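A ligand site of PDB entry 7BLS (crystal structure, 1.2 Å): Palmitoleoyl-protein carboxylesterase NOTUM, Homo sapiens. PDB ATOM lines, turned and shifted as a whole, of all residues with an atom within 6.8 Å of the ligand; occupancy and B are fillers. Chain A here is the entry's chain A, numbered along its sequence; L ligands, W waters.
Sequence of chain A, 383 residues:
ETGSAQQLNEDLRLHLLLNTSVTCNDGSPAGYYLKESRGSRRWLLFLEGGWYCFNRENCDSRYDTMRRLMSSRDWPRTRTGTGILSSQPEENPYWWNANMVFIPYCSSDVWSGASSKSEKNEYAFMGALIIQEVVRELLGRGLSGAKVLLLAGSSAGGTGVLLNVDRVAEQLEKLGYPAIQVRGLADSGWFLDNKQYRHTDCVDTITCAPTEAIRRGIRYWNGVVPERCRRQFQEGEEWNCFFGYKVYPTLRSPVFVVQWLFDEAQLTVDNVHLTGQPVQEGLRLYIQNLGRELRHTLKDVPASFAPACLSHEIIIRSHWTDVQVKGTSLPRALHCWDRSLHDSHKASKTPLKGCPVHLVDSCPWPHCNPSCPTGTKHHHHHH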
ATOM      1  N   GLU A  48      -2.635  16.889 -22.303  1.00  0.00           N
ATOM      2  CA  GLU A  48      -2.952  17.528 -21.046  1.00  0.00           C
ATOM      3  C   GLU A  48      -4.278  17.018 -20.483  1.00  0.00           C
ATOM      4  O   GLU A  48      -5.175  16.602 -21.229  1.00  0.00           O
ATOM      5  CB  GLU A  48      -3.055  19.037 -21.279  1.00  0.00           C
ATOM      6  CG  GLU A  48      -3.252  19.872 -20.035  1.00  0.00           C
ATOM      7  CD  GLU A  48      -3.483  21.335 -20.331  1.00  0.00           C
ATOM      8  OE1 GLU A  48      -3.886  21.672 -21.451  1.00  0.00           O
ATOM      9  OE2 GLU A  48      -3.262  22.179 -19.427  1.00  0.00           O
ATOM     10  N   GLY A  49      -4.409  17.052 -19.157  1.00  0.00           N
ATOM     11  CA  GLY A  49      -5.631  16.717 -18.474  1.00  0.00           C
ATOM     12  C   GLY A  49      -6.352  17.934 -17.935  1.00  0.00           C
ATOM     13  O   GLY A  49      -6.061  19.076 -18.289  1.00  0.00           O
ATOM     14  N   GLY A  50      -7.320  17.672 -17.053  1.00  0.00           N
ATOM     15  CA  GLY A  50      -8.104  18.717 -16.419  1.00  0.00           C
ATOM     16  C   GLY A  50      -9.613  18.502 -16.415  1.00  0.00           C
ATOM     17  O   GLY A  50     -10.375  19.404 -16.769  1.00  0.00           O
ATOM     18  N   TRP A  51     -10.049  17.324 -15.980  1.00  0.00           N
ATOM     19  CA  TRP A  51     -11.481  17.011 -15.785  1.00  0.00           C
ATOM     20  C   TRP A  51     -12.198  17.100 -17.134  1.00  0.00           C
ATOM     21  O   TRP A  51     -11.643  16.647 -18.147  1.00  0.00           O
ATOM     22  CB  TRP A  51     -12.095  17.812 -14.642  1.00  0.00           C
ATOM     23  CG  TRP A  51     -11.520  17.452 -13.323  1.00  0.00           C
ATOM     24  CD1 TRP A  51     -10.529  18.122 -12.672  1.00  0.00           C
ATOM     25  CD2 TRP A  51     -11.886  16.345 -12.498  1.00  0.00           C
ATOM     26  NE1 TRP A  51     -10.253  17.495 -11.473  1.00  0.00           N
ATOM     27  CE2 TRP A  51     -11.070  16.403 -11.347  1.00  0.00           C
ATOM     28  CE3 TRP A  51     -12.817  15.315 -12.616  1.00  0.00           C
ATOM     29  CZ2 TRP A  51     -11.166  15.461 -10.317  1.00  0.00           C
ATOM     30  CZ3 TRP A  51     -12.906  14.385 -11.589  1.00  0.00           C
ATOM     31  CH2 TRP A  51     -12.083  14.461 -10.450  1.00  0.00           C
ATOM     32  N   TYR A  52     -13.419  17.634 -17.165  1.00  0.00           N
ATOM     33  CA  TYR A  52     -14.314  17.612 -18.316  1.00  0.00           C
ATOM     34  C   TYR A  52     -15.547  18.410 -17.917  1.00  0.00           C
ATOM     35  O   TYR A  52     -15.697  18.787 -16.748  1.00  0.00           O
ATOM     36  CB  TYR A  52     -14.705  16.168 -18.723  1.00  0.00           C
ATOM     37  CG  TYR A  52     -15.189  15.316 -17.565  1.00  0.00           C
ATOM     38  CD1 TYR A  52     -16.510  15.368 -17.133  1.00  0.00           C
ATOM     39  CD2 TYR A  52     -14.328  14.454 -16.905  1.00  0.00           C
ATOM     40  CE1 TYR A  52     -16.943  14.595 -16.064  1.00  0.00           C
ATOM     41  CE2 TYR A  52     -14.759  13.669 -15.844  1.00  0.00           C
ATOM     42  CZ  TYR A  52     -16.067  13.752 -15.428  1.00  0.00           C
ATOM     43  OH  TYR A  52     -16.498  12.973 -14.375  1.00  0.00           O
ATOM     44  N   TYR A 105      -5.356  20.615 -23.732  1.00  0.00           N
ATOM     45  CA  TYR A 105      -6.690  20.064 -23.559  1.00  0.00           C
ATOM     46  C   TYR A 105      -7.663  21.234 -23.598  1.00  0.00           C
ATOM     47  O   TYR A 105      -7.753  22.016 -22.650  1.00  0.00           O
ATOM     48  CB  TYR A 105      -6.732  19.351 -22.210  1.00  0.00           C
ATOM     49  CG  TYR A 105      -8.009  18.655 -21.844  1.00  0.00           C
ATOM     50  CD1 TYR A 105      -8.753  17.955 -22.782  1.00  0.00           C
ATOM     51  CD2 TYR A 105      -8.420  18.636 -20.529  1.00  0.00           C
ATOM     52  CE1 TYR A 105      -9.909  17.282 -22.421  1.00  0.00           C
ATOM     53  CE2 TYR A 105      -9.563  17.952 -20.151  1.00  0.00           C
ATOM     54  CZ  TYR A 105     -10.309  17.286 -21.088  1.00  0.00           C
ATOM     55  OH  TYR A 105     -11.445  16.620 -20.721  1.00  0.00           O
ATOM     56  N   VAL A 110     -12.557  14.475 -22.290  1.00  0.00           N
ATOM     57  CA  VAL A 110     -11.651  13.362 -22.037  1.00  0.00           C
ATOM     58  C   VAL A 110     -11.040  12.905 -23.362  1.00  0.00           C
ATOM     59  O   VAL A 110     -10.726  11.720 -23.542  1.00  0.00           O
ATOM     60  CB  VAL A 110     -12.332  12.224 -21.246  1.00  0.00           C
ATOM     61  CG1 VAL A 110     -11.284  11.319 -20.599  1.00  0.00           C
ATOM     62  CG2 VAL A 110     -13.257  12.792 -20.185  1.00  0.00           C
ATOM     63  N   SER A 154      -1.661  12.829 -19.002  1.00  0.00           N
ATOM     64  CA  SER A 154      -1.896  12.805 -17.561  1.00  0.00           C
ATOM     65  C   SER A 154      -3.343  13.131 -17.242  1.00  0.00           C
ATOM     66  O   SER A 154      -3.946  14.010 -17.856  1.00  0.00           O
ATOM     67  CB  SER A 154      -0.997  13.798 -16.811  1.00  0.00           C
ATOM     68  OG  SER A 154       0.369  13.436 -16.947  1.00  0.00           O
ATOM     69  N   SER A 155      -3.881  12.435 -16.231  1.00  0.00           N
ATOM     70  CA  SER A 155      -5.239  12.692 -15.712  1.00  0.00           C
ATOM     71  C   SER A 155      -6.240  12.423 -16.826  1.00  0.00           C
ATOM     72  O   SER A 155      -6.208  11.331 -17.419  1.00  0.00           O
ATOM     73  CB  SER A 155      -5.300  14.071 -15.082  1.00  0.00           C
ATOM     74  OG  SER A 155      -4.293  14.228 -14.114  1.00  0.00           O
ATOM     75  N   ALA A 156      -7.126  13.359 -17.158  1.00  0.00           N
ATOM     76  CA  ALA A 156      -8.027  13.129 -18.289  1.00  0.00           C
ATOM     77  C   ALA A 156      -7.243  12.841 -19.558  1.00  0.00           C
ATOM     78  O   ALA A 156      -7.728  12.122 -20.427  1.00  0.00           O
ATOM     79  CB  ALA A 156      -8.941  14.350 -18.499  1.00  0.00           C
ATOM     80  N   GLY A 157      -6.026  13.390 -19.673  1.00  0.00           N
ATOM     81  CA  GLY A 157      -5.171  13.051 -20.803  1.00  0.00           C
ATOM     82  C   GLY A 157      -4.676  11.617 -20.764  1.00  0.00           C
ATOM     83  O   GLY A 157      -4.458  11.015 -21.822  1.00  0.00           O
ATOM     84  N   THR A 159      -6.514   9.053 -19.520  1.00  0.00           N
ATOM     85  CA  THR A 159      -7.664   8.345 -20.091  1.00  0.00           C
ATOM     86  C   THR A 159      -7.731   8.547 -21.597  1.00  0.00           C
ATOM     87  O   THR A 159      -8.022   7.617 -22.355  1.00  0.00           O
ATOM     88  CB  THR A 159      -8.944   8.817 -19.399  1.00  0.00           C
ATOM     89  OG1 THR A 159      -8.759   8.783 -17.976  1.00  0.00           O
ATOM     90  CG2 THR A 159     -10.134   7.930 -19.793  1.00  0.00           C
ATOM     91  N   SER A 188      -2.143   8.520 -14.514  1.00  0.00           N
ATOM     92  CA  SER A 188      -3.209   9.050 -13.660  1.00  0.00           C
ATOM     93  C   SER A 188      -4.561   9.081 -14.364  1.00  0.00           C
ATOM     94  O   SER A 188      -5.421   9.926 -14.054  1.00  0.00           O
ATOM     95  CB  SER A 188      -2.839  10.416 -13.100  1.00  0.00           C
ATOM     96  OG  SER A 188      -1.667  10.300 -12.290  1.00  0.00           O
ATOM     97  N   GLY A 189      -4.756   8.175 -15.312  1.00  0.00           N
ATOM     98  CA  GLY A 189      -6.018   8.072 -16.013  1.00  0.00           C
ATOM     99  C   GLY A 189      -6.673   6.716 -15.904  1.00  0.00           C
ATOM    100  O   GLY A 189      -7.534   6.390 -16.731  1.00  0.00           O
ATOM    101  N   PHE A 191      -8.969   4.697 -13.688  1.00  0.00           N
ATOM    102  CA  PHE A 191      -9.956   4.928 -12.642  1.00  0.00           C
ATOM    103  C   PHE A 191     -10.815   3.699 -12.432  1.00  0.00           C
ATOM    104  O   PHE A 191     -10.966   2.846 -13.315  1.00  0.00           O
ATOM    105  CB  PHE A 191     -10.851   6.118 -13.010  1.00  0.00           C
ATOM    106  CG  PHE A 191     -10.076   7.388 -13.155  1.00  0.00           C
ATOM    107  CD1 PHE A 191      -9.886   7.973 -14.395  1.00  0.00           C
ATOM    108  CD2 PHE A 191      -9.449   7.941 -12.056  1.00  0.00           C
ATOM    109  CE1 PHE A 191      -9.136   9.138 -14.519  1.00  0.00           C
ATOM    110  CE2 PHE A 191      -8.706   9.099 -12.184  1.00  0.00           C
ATOM    111  CZ  PHE A 191      -8.545   9.701 -13.426  1.00  0.00           C
ATOM    112  N   LEU A 192     -11.379   3.611 -11.222  1.00  0.00           N
ATOM    113  CA  LEU A 192     -12.306   2.550 -10.854  1.00  0.00           C
ATOM    114  C   LEU A 192     -13.720   3.107 -10.774  1.00  0.00           C
ATOM    115  O   LEU A 192     -13.942   4.167 -10.173  1.00  0.00           O
ATOM    116  CB  LEU A 192     -11.936   1.959  -9.488  1.00  0.00           C
ATOM    117  CG  LEU A 192     -10.512   1.411  -9.399  1.00  0.00           C
ATOM    118  CD1 LEU A 192     -10.263   0.820  -8.037  1.00  0.00           C
ATOM    119  CD2 LEU A 192     -10.238   0.379 -10.499  1.00  0.00           C
ATOM    120  N   PRO A 210     -18.743   9.697 -11.830  1.00  0.00           N
ATOM    121  CA  PRO A 210     -18.178   9.666 -13.189  1.00  0.00           C
ATOM    122  C   PRO A 210     -18.903   8.748 -14.151  1.00  0.00           C
ATOM    123  O   PRO A 210     -19.027   9.104 -15.322  1.00  0.00           O
ATOM    124  CB  PRO A 210     -16.732   9.209 -12.970  1.00  0.00           C
ATOM    125  CG  PRO A 210     -16.427   9.580 -11.593  1.00  0.00           C
ATOM    126  CD  PRO A 210     -17.709   9.501 -10.809  1.00  0.00           C
ATOM    127  N   ILE A 214     -20.036  10.601 -17.308  1.00  0.00           N
ATOM    128  CA  ILE A 214     -19.472  10.169 -18.578  1.00  0.00           C
ATOM    129  C   ILE A 214     -20.558   9.662 -19.522  1.00  0.00           C
ATOM    130  O   ILE A 214     -20.520   9.933 -20.725  1.00  0.00           O
ATOM    131  CB  ILE A 214     -18.361   9.125 -18.356  1.00  0.00           C
ATOM    132  CG1 ILE A 214     -17.158   9.810 -17.699  1.00  0.00           C
ATOM    133  CG2 ILE A 214     -17.934   8.468 -19.659  1.00  0.00           C
ATOM    134  CD1 ILE A 214     -16.148   8.819 -17.167  1.00  0.00           C
ATOM    135  N   PHE A 242     -14.233   4.133 -20.762  1.00  0.00           N
ATOM    136  CA  PHE A 242     -13.435   5.164 -20.112  1.00  0.00           C
ATOM    137  C   PHE A 242     -12.704   4.639 -18.885  1.00  0.00           C
ATOM    138  O   PHE A 242     -11.912   5.382 -18.287  1.00  0.00           O
ATOM    139  CB  PHE A 242     -14.324   6.341 -19.695  1.00  0.00           C
ATOM    140  CG  PHE A 242     -14.696   7.275 -20.833  1.00  0.00           C
ATOM    141  CD1 PHE A 242     -15.398   6.828 -21.944  1.00  0.00           C
ATOM    142  CD2 PHE A 242     -14.387   8.623 -20.749  1.00  0.00           C
ATOM    143  CE1 PHE A 242     -15.746   7.703 -22.975  1.00  0.00           C
ATOM    144  CE2 PHE A 242     -14.750   9.496 -21.757  1.00  0.00           C
ATOM    145  CZ  PHE A 242     -15.416   9.046 -22.869  1.00  0.00           C
ATOM    146  N   PHE A 243     -12.958   3.395 -18.493  1.00  0.00           N
ATOM    147  CA  PHE A 243     -12.348   2.789 -17.317  1.00  0.00           C
ATOM    148  C   PHE A 243     -11.242   1.848 -17.739  1.00  0.00           C
ATOM    149  O   PHE A 243     -11.486   0.854 -18.418  1.00  0.00           O
ATOM    150  CB  PHE A 243     -13.430   2.123 -16.463  1.00  0.00           C
ATOM    151  CG  PHE A 243     -14.312   3.146 -15.836  1.00  0.00           C
ATOM    152  CD1 PHE A 243     -15.403   3.645 -16.522  1.00  0.00           C
ATOM    153  CD2 PHE A 243     -13.956   3.725 -14.627  1.00  0.00           C
ATOM    154  CE1 PHE A 243     -16.173   4.658 -15.974  1.00  0.00           C
ATOM    155  CE2 PHE A 243     -14.712   4.744 -14.086  1.00  0.00           C
ATOM    156  CZ  PHE A 243     -15.823   5.207 -14.762  1.00  0.00           C
ATOM    157  N   ASP A 263      -5.074   7.735  -5.926  1.00  0.00           N
ATOM    158  CA  ASP A 263      -5.101   8.916  -6.771  1.00  0.00           C
ATOM    159  C   ASP A 263      -6.097   9.942  -6.245  1.00  0.00           C
ATOM    160  O   ASP A 263      -7.226   9.606  -5.883  1.00  0.00           O
ATOM    161  CB  ASP A 263      -5.465   8.508  -8.190  1.00  0.00           C
ATOM    162  CG  ASP A 263      -5.442   9.664  -9.114  1.00  0.00           C
ATOM    163  OD1 ASP A 263      -4.347  10.007  -9.609  1.00  0.00           O
ATOM    164  OD2 ASP A 263      -6.525  10.248  -9.340  1.00  0.00           O
ATOM    165  N   ALA A 265      -7.773  12.312  -7.733  1.00  0.00           N
ATOM    166  CA  ALA A 265      -8.997  12.431  -8.517  1.00  0.00           C
ATOM    167  C   ALA A 265      -9.950  11.278  -8.230  1.00  0.00           C
ATOM    168  O   ALA A 265     -11.176  11.468  -8.154  1.00  0.00           O
ATOM    169  CB  ALA A 265      -8.685  12.541 -10.005  1.00  0.00           C
ATOM    170  N   GLN A 266      -9.408  10.064  -8.089  1.00  0.00           N
ATOM    171  CA  GLN A 266     -10.233   8.920  -7.692  1.00  0.00           C
ATOM    172  C   GLN A 266     -10.893   9.160  -6.342  1.00  0.00           C
ATOM    173  O   GLN A 266     -12.093   8.928  -6.166  1.00  0.00           O
ATOM    174  CB  GLN A 266      -9.358   7.664  -7.620  1.00  0.00           C
ATOM    175  CG  GLN A 266     -10.102   6.414  -7.199  1.00  0.00           C
ATOM    176  CD  GLN A 266     -10.962   5.833  -8.301  1.00  0.00           C
ATOM    177  OE1 GLN A 266     -10.481   5.609  -9.421  1.00  0.00           O
ATOM    178  NE2 GLN A 266     -12.225   5.579  -8.008  1.00  0.00           N
ATOM    179  N   VAL A 269     -13.835  11.690  -6.709  1.00  0.00           N
ATOM    180  CA  VAL A 269     -15.081  11.150  -7.234  1.00  0.00           C
ATOM    181  C   VAL A 269     -15.676  10.100  -6.312  1.00  0.00           C
ATOM    182  O   VAL A 269     -16.867   9.781  -6.424  1.00  0.00           O
ATOM    183  CB  VAL A 269     -14.928  10.633  -8.679  1.00  0.00           C
ATOM    184  CG1 VAL A 269     -14.458  11.758  -9.587  1.00  0.00           C
ATOM    185  CG2 VAL A 269     -13.983   9.429  -8.729  1.00  0.00           C
ATOM    186  N   HIS A 312      -1.372  12.941  -7.560  1.00  0.00           N
ATOM    187  CA  HIS A 312      -2.113  13.097  -8.812  1.00  0.00           C
ATOM    188  C   HIS A 312      -1.148  13.554  -9.898  1.00  0.00           C
ATOM    189  O   HIS A 312      -0.510  14.604  -9.737  1.00  0.00           O
ATOM    190  CB  HIS A 312      -3.197  14.158  -8.598  1.00  0.00           C
ATOM    191  CG  HIS A 312      -4.120  14.310  -9.759  1.00  0.00           C
ATOM    192  ND1 HIS A 312      -4.325  15.525 -10.398  1.00  0.00           N
ATOM    193  CD2 HIS A 312      -4.918  13.417 -10.394  1.00  0.00           C
ATOM    194  CE1 HIS A 312      -5.211  15.357 -11.371  1.00  0.00           C
ATOM    195  NE2 HIS A 312      -5.578  14.086 -11.389  1.00  0.00           N
ATOM    196  N   GLU A 313      -1.042  12.774 -10.980  1.00  0.00           N
ATOM    197  CA  GLU A 313      -0.121  13.022 -12.098  1.00  0.00           C
ATOM    198  C   GLU A 313       1.325  12.775 -11.698  1.00  0.00           C
ATOM    199  O   GLU A 313       1.657  12.816 -10.514  1.00  0.00           O
ATOM    200  CB  GLU A 313      -0.271  14.413 -12.717  1.00  0.00           C
ATOM    201  CG  GLU A 313      -1.695  14.809 -13.017  1.00  0.00           C
ATOM    202  CD  GLU A 313      -1.823  16.100 -13.797  1.00  0.00           C
ATOM    203  OE1 GLU A 313      -1.053  17.045 -13.535  1.00  0.00           O
ATOM    204  OE2 GLU A 313      -2.711  16.173 -14.692  1.00  0.00           O
HETATM  205  N1  LIG L   1     -12.230  11.288 -16.426  1.00  0.00           N
HETATM  206  C1  LIG L   1     -12.736  10.169 -14.309  1.00  0.00           C
HETATM  207  C2  LIG L   1     -12.572  10.026 -12.930  1.00  0.00           C
HETATM  208  C3  LIG L   1     -11.687  10.876 -12.299  1.00  0.00           C
HETATM  209  C4  LIG L   1     -11.146  11.953 -14.259  1.00  0.00           C
HETATM  210  C5  LIG L   1      -9.245  13.937 -13.568  1.00  0.00           C
HETATM  211  C6  LIG L   1      -8.332  15.073 -13.993  1.00  0.00           C
HETATM  212  C7  LIG L   1     -12.005  11.134 -14.990  1.00  0.00           C
HETATM  213  N2  LIG L   1     -11.012  11.804 -12.961  1.00  0.00           N
HETATM  214  O1  LIG L   1      -8.225  15.401 -15.215  1.00  0.00           O
HETATM  215  O2  LIG L   1      -7.658  15.679 -13.114  1.00  0.00           O
HETATM  216  O3  LIG L   1     -12.364  10.264 -17.024  1.00  0.00           O
HETATM  217  O4  LIG L   1     -11.327  12.201 -16.979  1.00  0.00           O
HETATM  218  S1  LIG L   1     -10.121  13.268 -15.009  1.00  0.00           S
HETATM  219  O   HOH W   1      -6.284  17.705 -13.614  1.00  0.00           O
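The backbone NH of Trp 51 is in hydrogen-bond range of an oxygen (O1) of the ligand, at 2.8 Å. The backbone NH of Gly 50 sits at hydrogen-bond distance from an oxygen (O1) of the ligand (3.1 Å). An oxygen (O1) of the ligand lies within hydrogen-bond range of the backbone NH (N) of Ala 156 (3.0 Å). NE2 of His 312 lies close to O2 of the ligand (3.1 Å).
O of Trp 51 lies within hydrogen-bond range of OH of Tyr 105. The side-chain carboxylate (OE2) of Glu 313 lies within hydrogen-bond range of the side-chain hydroxyl (OG) of Ser 155, 2.6 Å away. The side-chain hydroxyl of Ser 155 lies within hydrogen-bond range of a ring nitrogen (NE2) of His 312, at 3.0 Å. The side-chain carboxylate (OD2) of Asp 263 is in hydrogen-bond range of the backbone NH (N) of Ala 265, at 2.9 Å. The backbone NH (N) of Val 110 is in hydrogen-bond range of the side-chain hydroxyl (OH) of Tyr 105, 2.9 Å away.
Merely in contact with the ligand: Ser 155 (3.2 Å), Phe 191 (3.3 Å), Tyr 52 (3.5 Å), Val 110 (3.7 Å), Ala 265 (3.8 Å) and Val 269 (3.98 Å). Hydrophobic or aromatic side chains within 4 Å of the ligand: Trp 51, Tyr 52, Val 110, Ala 156, Phe 191, Ala 265, Val 269 and His 312. Within 4 Å of the ligand: Gly 50, Trp 51, Tyr 52, Val 110, Ser 155, Ala 156, Phe 191, Ala 265, Val 269 and His 312.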
